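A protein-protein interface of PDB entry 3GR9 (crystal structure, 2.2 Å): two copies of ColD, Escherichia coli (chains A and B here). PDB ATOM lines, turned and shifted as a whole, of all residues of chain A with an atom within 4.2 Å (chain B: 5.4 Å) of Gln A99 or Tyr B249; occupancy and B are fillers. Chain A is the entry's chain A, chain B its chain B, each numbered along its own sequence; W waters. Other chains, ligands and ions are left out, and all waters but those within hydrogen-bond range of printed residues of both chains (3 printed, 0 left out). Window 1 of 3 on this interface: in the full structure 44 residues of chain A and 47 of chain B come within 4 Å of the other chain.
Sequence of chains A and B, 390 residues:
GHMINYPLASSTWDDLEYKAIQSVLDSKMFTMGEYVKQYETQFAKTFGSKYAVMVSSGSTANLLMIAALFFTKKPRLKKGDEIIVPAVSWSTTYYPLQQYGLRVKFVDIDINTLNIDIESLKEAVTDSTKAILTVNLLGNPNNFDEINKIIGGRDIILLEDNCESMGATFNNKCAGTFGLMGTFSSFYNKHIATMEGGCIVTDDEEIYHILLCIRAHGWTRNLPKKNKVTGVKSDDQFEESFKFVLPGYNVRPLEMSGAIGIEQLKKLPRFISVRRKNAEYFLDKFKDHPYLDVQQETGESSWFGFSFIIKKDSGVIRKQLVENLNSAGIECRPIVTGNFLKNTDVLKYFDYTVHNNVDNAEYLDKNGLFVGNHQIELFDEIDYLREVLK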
ATOM      1  N   TYR A  95      21.950  26.949   1.826  1.00  0.00           N
ATOM      2  CA  TYR A  95      22.767  26.562   0.690  1.00  0.00           C
ATOM      3  C   TYR A  95      22.002  26.139  -0.572  1.00  0.00           C
ATOM      4  O   TYR A  95      22.361  26.438  -1.712  1.00  0.00           O
ATOM      5  CB  TYR A  95      23.611  25.397   1.145  1.00  0.00           C
ATOM      6  CG  TYR A  95      24.585  25.777   2.216  1.00  0.00           C
ATOM      7  CD1 TYR A  95      24.715  27.104   2.618  1.00  0.00           C
ATOM      8  CD2 TYR A  95      25.398  24.817   2.817  1.00  0.00           C
ATOM      9  CE1 TYR A  95      25.672  27.467   3.548  1.00  0.00           C
ATOM     10  CE2 TYR A  95      26.344  25.178   3.761  1.00  0.00           C
ATOM     11  CZ  TYR A  95      26.469  26.498   4.123  1.00  0.00           C
ATOM     12  OH  TYR A  95      27.400  26.876   5.069  1.00  0.00           O
ATOM     13  N   PRO A  96      20.957  25.370  -0.345  1.00  0.00           N
ATOM     14  CA  PRO A  96      20.131  24.889  -1.431  1.00  0.00           C
ATOM     15  C   PRO A  96      19.581  26.035  -2.279  1.00  0.00           C
ATOM     16  O   PRO A  96      19.407  25.915  -3.526  1.00  0.00           O
ATOM     17  CB  PRO A  96      18.991  24.139  -0.673  1.00  0.00           C
ATOM     18  CG  PRO A  96      19.853  23.493   0.605  1.00  0.00           C
ATOM     19  CD  PRO A  96      20.697  24.692   0.953  1.00  0.00           C
ATOM     20  N   LEU A  97      19.204  27.148  -1.640  1.00  0.00           N
ATOM     21  CA  LEU A  97      18.611  28.234  -2.393  1.00  0.00           C
ATOM     22  C   LEU A  97      19.719  28.837  -3.193  1.00  0.00           C
ATOM     23  O   LEU A  97      19.542  29.235  -4.334  1.00  0.00           O
ATOM     24  CB  LEU A  97      18.053  29.270  -1.421  1.00  0.00           C
ATOM     25  CG  LEU A  97      17.495  28.601  -0.162  1.00  0.00           C
ATOM     26  CD1 LEU A  97      17.383  29.589   0.959  1.00  0.00           C
ATOM     27  CD2 LEU A  97      16.138  27.953  -0.380  1.00  0.00           C
ATOM     28  N   GLN A  98      20.883  28.905  -2.572  1.00  0.00           N
ATOM     29  CA  GLN A  98      22.026  29.519  -3.242  1.00  0.00           C
ATOM     30  C   GLN A  98      22.397  28.568  -4.335  1.00  0.00           C
ATOM     31  O   GLN A  98      22.605  28.968  -5.495  1.00  0.00           O
ATOM     32  CB  GLN A  98      23.211  29.691  -2.268  1.00  0.00           C
ATOM     33  CG  GLN A  98      24.398  30.436  -2.891  1.00  0.00           C
ATOM     34  CD  GLN A  98      25.197  29.529  -3.807  1.00  0.00           C
ATOM     35  OE1 GLN A  98      25.225  28.306  -3.557  1.00  0.00           O
ATOM     36  NE2 GLN A  98      25.876  30.097  -4.860  1.00  0.00           N
ATOM     37  N   GLN A  99      22.450  27.284  -3.996  1.00  0.00           N
ATOM     38  CA  GLN A  99      22.821  26.319  -5.015  1.00  0.00           C
ATOM     39  C   GLN A  99      21.815  26.241  -6.148  1.00  0.00           C
ATOM     40  O   GLN A  99      22.179  25.838  -7.259  1.00  0.00           O
ATOM     41  CB  GLN A  99      23.201  24.966  -4.413  1.00  0.00           C
ATOM     42  CG  GLN A  99      24.221  25.104  -3.292  1.00  0.00           C
ATOM     43  CD  GLN A  99      24.186  23.975  -2.265  1.00  0.00           C
ATOM     44  OE1 GLN A  99      23.132  23.438  -1.936  1.00  0.00           O
ATOM     45  NE2 GLN A  99      25.350  23.658  -1.712  1.00  0.00           N
ATOM     46  N   TYR A 100      20.589  26.705  -5.907  1.00  0.00           N
ATOM     47  CA  TYR A 100      19.571  26.658  -6.947  1.00  0.00           C
ATOM     48  C   TYR A 100      19.324  27.923  -7.735  1.00  0.00           C
ATOM     49  O   TYR A 100      18.523  27.934  -8.686  1.00  0.00           O
ATOM     50  CB  TYR A 100      18.312  25.933  -6.494  1.00  0.00           C
ATOM     51  CG  TYR A 100      18.471  24.454  -6.753  1.00  0.00           C
ATOM     52  CD1 TYR A 100      19.142  23.654  -5.855  1.00  0.00           C
ATOM     53  CD2 TYR A 100      18.096  23.902  -7.960  1.00  0.00           C
ATOM     54  CE1 TYR A 100      19.391  22.330  -6.125  1.00  0.00           C
ATOM     55  CE2 TYR A 100      18.319  22.579  -8.235  1.00  0.00           C
ATOM     56  CZ  TYR A 100      18.995  21.801  -7.323  1.00  0.00           C
ATOM     57  OH  TYR A 100      19.274  20.483  -7.585  1.00  0.00           O
ATOM     58  N   GLY A 101      20.043  28.976  -7.347  1.00  0.00           N
ATOM     59  CA  GLY A 101      19.966  30.264  -8.040  1.00  0.00           C
ATOM     60  C   GLY A 101      18.756  31.119  -7.690  1.00  0.00           C
ATOM     61  O   GLY A 101      18.325  31.986  -8.474  1.00  0.00           O
ATOM     62  N   LEU B  63      30.106  15.223  -7.111  1.00  0.00           N
ATOM     63  CA  LEU B  63      29.474  16.514  -6.798  1.00  0.00           C
ATOM     64  C   LEU B  63      30.507  17.457  -6.207  1.00  0.00           C
ATOM     65  O   LEU B  63      30.686  18.587  -6.637  1.00  0.00           O
ATOM     66  CB  LEU B  63      28.387  16.288  -5.747  1.00  0.00           C
ATOM     67  CG  LEU B  63      27.627  17.501  -5.230  1.00  0.00           C
ATOM     68  CD1 LEU B  63      27.251  18.409  -6.371  1.00  0.00           C
ATOM     69  CD2 LEU B  63      26.370  17.027  -4.515  1.00  0.00           C
ATOM     70  N   LEU B  64      31.170  16.961  -5.177  1.00  0.00           N
ATOM     71  CA  LEU B  64      32.212  17.669  -4.487  1.00  0.00           C
ATOM     72  C   LEU B  64      33.409  17.934  -5.378  1.00  0.00           C
ATOM     73  O   LEU B  64      33.899  19.074  -5.452  1.00  0.00           O
ATOM     74  CB  LEU B  64      32.587  16.906  -3.225  1.00  0.00           C
ATOM     75  CG  LEU B  64      31.885  17.603  -2.035  1.00  0.00           C
ATOM     76  CD1 LEU B  64      30.336  17.732  -2.136  1.00  0.00           C
ATOM     77  CD2 LEU B  64      32.257  16.963  -0.725  1.00  0.00           C
ATOM     78  N   ALA B  67      31.966  21.038  -7.393  1.00  0.00           N
ATOM     79  CA  ALA B  67      31.703  22.200  -6.544  1.00  0.00           C
ATOM     80  C   ALA B  67      33.005  22.824  -6.126  1.00  0.00           C
ATOM     81  O   ALA B  67      33.166  24.047  -6.115  1.00  0.00           O
ATOM     82  CB  ALA B  67      30.979  21.799  -5.281  1.00  0.00           C
ATOM     83  N   GLN B  99      24.601  20.912 -12.762  1.00  0.00           N
ATOM     84  CA  GLN B  99      24.166  21.564 -11.529  1.00  0.00           C
ATOM     85  C   GLN B  99      24.971  22.804 -11.210  1.00  0.00           C
ATOM     86  O   GLN B  99      24.492  23.755 -10.605  1.00  0.00           O
ATOM     87  CB  GLN B  99      24.084  20.570 -10.371  1.00  0.00           C
ATOM     88  CG  GLN B  99      22.871  19.611 -10.410  1.00  0.00           C
ATOM     89  CD  GLN B  99      23.155  18.219  -9.913  1.00  0.00           C
ATOM     90  OE1 GLN B  99      24.333  17.857  -9.676  1.00  0.00           O
ATOM     91  NE2 GLN B  99      22.107  17.432  -9.706  1.00  0.00           N
ATOM     92  N   TYR B 100      26.199  22.781 -11.704  1.00  0.00           N
ATOM     93  CA  TYR B 100      27.090  23.904 -11.562  1.00  0.00           C
ATOM     94  C   TYR B 100      27.123  24.798 -12.789  1.00  0.00           C
ATOM     95  O   TYR B 100      27.998  25.654 -12.906  1.00  0.00           O
ATOM     96  CB  TYR B 100      28.480  23.453 -11.138  1.00  0.00           C
ATOM     97  CG  TYR B 100      28.492  23.257  -9.659  1.00  0.00           C
ATOM     98  CD1 TYR B 100      27.911  22.134  -9.108  1.00  0.00           C
ATOM     99  CD2 TYR B 100      28.904  24.274  -8.802  1.00  0.00           C
ATOM    100  CE1 TYR B 100      27.838  21.968  -7.763  1.00  0.00           C
ATOM    101  CE2 TYR B 100      28.853  24.109  -7.437  1.00  0.00           C
ATOM    102  CZ  TYR B 100      28.307  22.945  -6.933  1.00  0.00           C
ATOM    103  OH  TYR B 100      28.181  22.741  -5.597  1.00  0.00           O
ATOM    104  N   ILE B 214      33.503  21.651   2.601  1.00  0.00           N
ATOM    105  CA  ILE B 214      32.238  21.447   1.927  1.00  0.00           C
ATOM    106  C   ILE B 214      31.528  20.118   2.104  1.00  0.00           C
ATOM    107  O   ILE B 214      30.338  20.021   1.825  1.00  0.00           O
ATOM    108  CB  ILE B 214      32.166  22.004   0.496  1.00  0.00           C
ATOM    109  CG1 ILE B 214      32.952  21.148  -0.500  1.00  0.00           C
ATOM    110  CG2 ILE B 214      32.478  23.496   0.408  1.00  0.00           C
ATOM    111  CD1 ILE B 214      32.712  21.645  -1.904  1.00  0.00           C
ATOM    112  N   ARG B 215      32.246  19.110   2.585  1.00  0.00           N
ATOM    113  CA  ARG B 215      31.626  17.801   2.821  1.00  0.00           C
ATOM    114  C   ARG B 215      30.665  17.886   4.005  1.00  0.00           C
ATOM    115  O   ARG B 215      29.663  17.120   4.039  1.00  0.00           O
ATOM    116  CB  ARG B 215      32.690  16.787   3.226  1.00  0.00           C
ATOM    117  CG  ARG B 215      32.116  15.525   3.862  1.00  0.00           C
ATOM    118  CD  ARG B 215      33.175  14.430   4.084  1.00  0.00           C
ATOM    119  NE  ARG B 215      34.102  14.757   5.170  1.00  0.00           N
ATOM    120  CZ  ARG B 215      35.193  14.049   5.452  1.00  0.00           C
ATOM    121  NH1 ARG B 215      35.519  12.969   4.723  1.00  0.00           N
ATOM    122  NH2 ARG B 215      35.955  14.438   6.443  1.00  0.00           N
ATOM    123  N   ALA B 216      30.938  18.810   4.940  1.00  0.00           N
ATOM    124  CA  ALA B 216      30.103  18.904   6.117  1.00  0.00           C
ATOM    125  C   ALA B 216      29.637  20.289   6.502  1.00  0.00           C
ATOM    126  O   ALA B 216      30.292  20.952   7.325  1.00  0.00           O
ATOM    127  CB  ALA B 216      30.837  18.287   7.267  1.00  0.00           C
ATOM    128  N   HIS B 217      28.502  20.715   5.946  1.00  0.00           N
ATOM    129  CA  HIS B 217      27.902  21.986   6.349  1.00  0.00           C
ATOM    130  C   HIS B 217      28.618  23.314   6.044  1.00  0.00           C
ATOM    131  O   HIS B 217      28.077  24.372   6.374  1.00  0.00           O
ATOM    132  CB  HIS B 217      27.522  21.926   7.872  1.00  0.00           C
ATOM    133  CG  HIS B 217      26.709  20.716   8.248  1.00  0.00           C
ATOM    134  ND1 HIS B 217      25.382  20.583   7.905  1.00  0.00           N
ATOM    135  CD2 HIS B 217      27.050  19.562   8.879  1.00  0.00           C
ATOM    136  CE1 HIS B 217      24.933  19.408   8.313  1.00  0.00           C
ATOM    137  NE2 HIS B 217      25.932  18.768   8.908  1.00  0.00           N
ATOM    138  N   GLY B 218      29.819  23.291   5.463  1.00  0.00           N
ATOM    139  CA  GLY B 218      30.532  24.553   5.170  1.00  0.00           C
ATOM    140  C   GLY B 218      30.985  25.255   6.465  1.00  0.00           C
ATOM    141  O   GLY B 218      31.200  26.463   6.479  1.00  0.00           O
ATOM    142  N   PRO B 247      29.263  27.355   0.966  1.00  0.00           N
ATOM    143  CA  PRO B 247      27.957  26.696   0.740  1.00  0.00           C
ATOM    144  C   PRO B 247      28.290  25.256   0.384  1.00  0.00           C
ATOM    145  O   PRO B 247      28.744  24.940  -0.722  1.00  0.00           O
ATOM    146  CB  PRO B 247      27.335  27.462  -0.451  1.00  0.00           C
ATOM    147  CG  PRO B 247      28.426  28.491  -0.949  1.00  0.00           C
ATOM    148  CD  PRO B 247      29.730  28.139  -0.193  1.00  0.00           C
ATOM    149  N   GLY B 248      28.097  24.388   1.350  1.00  0.00           N
ATOM    150  CA  GLY B 248      28.411  22.997   1.172  1.00  0.00           C
ATOM    151  C   GLY B 248      27.176  22.150   1.211  1.00  0.00           C
ATOM    152  O   GLY B 248      26.099  22.558   0.827  1.00  0.00           O
ATOM    153  N   TYR B 249      27.377  20.951   1.707  1.00  0.00           N
ATOM    154  CA  TYR B 249      26.379  19.935   1.754  1.00  0.00           C
ATOM    155  C   TYR B 249      26.631  19.154   3.011  1.00  0.00           C
ATOM    156  O   TYR B 249      27.642  19.343   3.660  1.00  0.00           O
ATOM    157  CB  TYR B 249      26.611  19.002   0.571  1.00  0.00           C
ATOM    158  CG  TYR B 249      26.483  19.637  -0.783  1.00  0.00           C
ATOM    159  CD1 TYR B 249      25.249  19.946  -1.300  1.00  0.00           C
ATOM    160  CD2 TYR B 249      27.597  19.912  -1.551  1.00  0.00           C
ATOM    161  CE1 TYR B 249      25.116  20.511  -2.534  1.00  0.00           C
ATOM    162  CE2 TYR B 249      27.484  20.483  -2.788  1.00  0.00           C
ATOM    163  CZ  TYR B 249      26.234  20.775  -3.280  1.00  0.00           C
ATOM    164  OH  TYR B 249      26.086  21.347  -4.499  1.00  0.00           O
ATOM    165  N   ASN B 250      25.733  18.242   3.350  1.00  0.00           N
ATOM    166  CA  ASN B 250      26.075  17.311   4.398  1.00  0.00           C
ATOM    167  C   ASN B 250      26.365  15.959   3.772  1.00  0.00           C
ATOM    168  O   ASN B 250      25.493  15.099   3.756  1.00  0.00           O
ATOM    169  CB  ASN B 250      25.017  17.167   5.483  1.00  0.00           C
ATOM    170  CG  ASN B 250      25.245  15.938   6.323  1.00  0.00           C
ATOM    171  OD1 ASN B 250      26.148  15.172   6.045  1.00  0.00           O
ATOM    172  ND2 ASN B 250      24.443  15.744   7.342  1.00  0.00           N
ATOM    173  N   VAL B 251      27.578  15.779   3.255  1.00  0.00           N
ATOM    174  CA  VAL B 251      27.972  14.513   2.610  1.00  0.00           C
ATOM    175  C   VAL B 251      28.847  13.516   3.309  1.00  0.00           C
ATOM    176  O   VAL B 251      29.466  12.645   2.682  1.00  0.00           O
ATOM    177  CB  VAL B 251      28.004  14.470   1.072  1.00  0.00           C
ATOM    178  CG1 VAL B 251      26.750  15.100   0.523  1.00  0.00           C
ATOM    179  CG2 VAL B 251      29.297  15.063   0.457  1.00  0.00           C
HETATM  180  O   HOH W   1      23.150  21.951   0.093  1.00  0.00           O
HETATM  181  O   HOH W   2      19.359  18.915 -10.061  1.00  0.00           O
HETATM  182  O   HOH W   3      28.017  24.544  -3.506  1.00  0.00           O
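Positions printed for both chains: 99 and 100. Of the 8 pairs that touch across the chains among the printed residues, none has its exchanged pair printed and touching as well.
Of the printed residues of chain B, Gln A98 touches Pro B247 (3.8 Å). Gln A99 touches just these residues of chain B: Pro B247 (3.8 Å), Gly B248 (2.9 Å) and Tyr B249 (3.3 Å). Printed residues of chain A within 4 Å of Pro B247: Tyr A95, Gln A98 and Gln A99. Of chain A, only Gln A99 (3.3 Å) comes within 4 Å of Tyr B249. The nearest residue of chain B that does not touch Gln A99 is Gln B99 (4.6 Å).
Among the printed residues, merely in contact across the chains: Tyr A95 with Gly B218, Tyr A95 with Pro B247, Tyr A95 with Gly B248, Gln A98 with Pro B247, Gln A99 with Pro B247 and Gln A99 with Tyr B249.
Water W1 bridges the side-chain amide oxygen (OE1) of Gln A99 (2.5 Å) and the backbone carbonyl oxygen (O) of Gly B248 (3.1 Å). Water W3 lies within hydrogen-bond range of the side-chain hydroxyl of Tyr B100 (2.8 Å), the backbone carbonyl oxygen of Pro B247 (2.9 Å) and the side-chain amide nitrogen of Gln A99 (3.3 Å). Water W2 bridges OH of Tyr A100 (2.9 Å) and NE2 of Gln B99 (3.1 Å).
The side-chain hydroxyl (OH) of Tyr A95 is in hydrogen-bond range of the backbone carbonyl oxygen (O) of His B217 (2.9 Å). The backbone carbonyl oxygen (O) of Gly B248 is in hydrogen-bond range of the side-chain amide nitrogen (NE2) of Gln A99.
The backbone carbonyl oxygen (O) of Tyr A95 lies close to the side-chain amide oxygen (OE1) of Gln A99. The side-chain hydroxyl (OH) of Tyr B100 lies within hydrogen-bond range of the side-chain hydroxyl (OH) of Tyr B249, at 2.7 Å. O of Ile B214 sits at hydrogen-bond distance from N of Tyr B249, 3.1 Å away. The backbone carbonyl oxygen (O) of Tyr B249 lies within hydrogen-bond range of the backbone NH (N) of His B217.
Of the 7 printed residues of chain A, 3 touch a printed residue of chain B. Hydrophobic or aromatic side chains of chain A that line the printed part of chain B: Tyr A95. Of the 15 printed residues of chain B, 5 touch a printed residue of chain A. Hydrophobic or aromatic side chains of chain B that line the printed part of chain A: Pro B247 and Tyr B249. Among the printed residues, no Asp or Glu carboxylate lies within 4 Å of a Lys or Arg side-chain nitrogen of the other chain.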
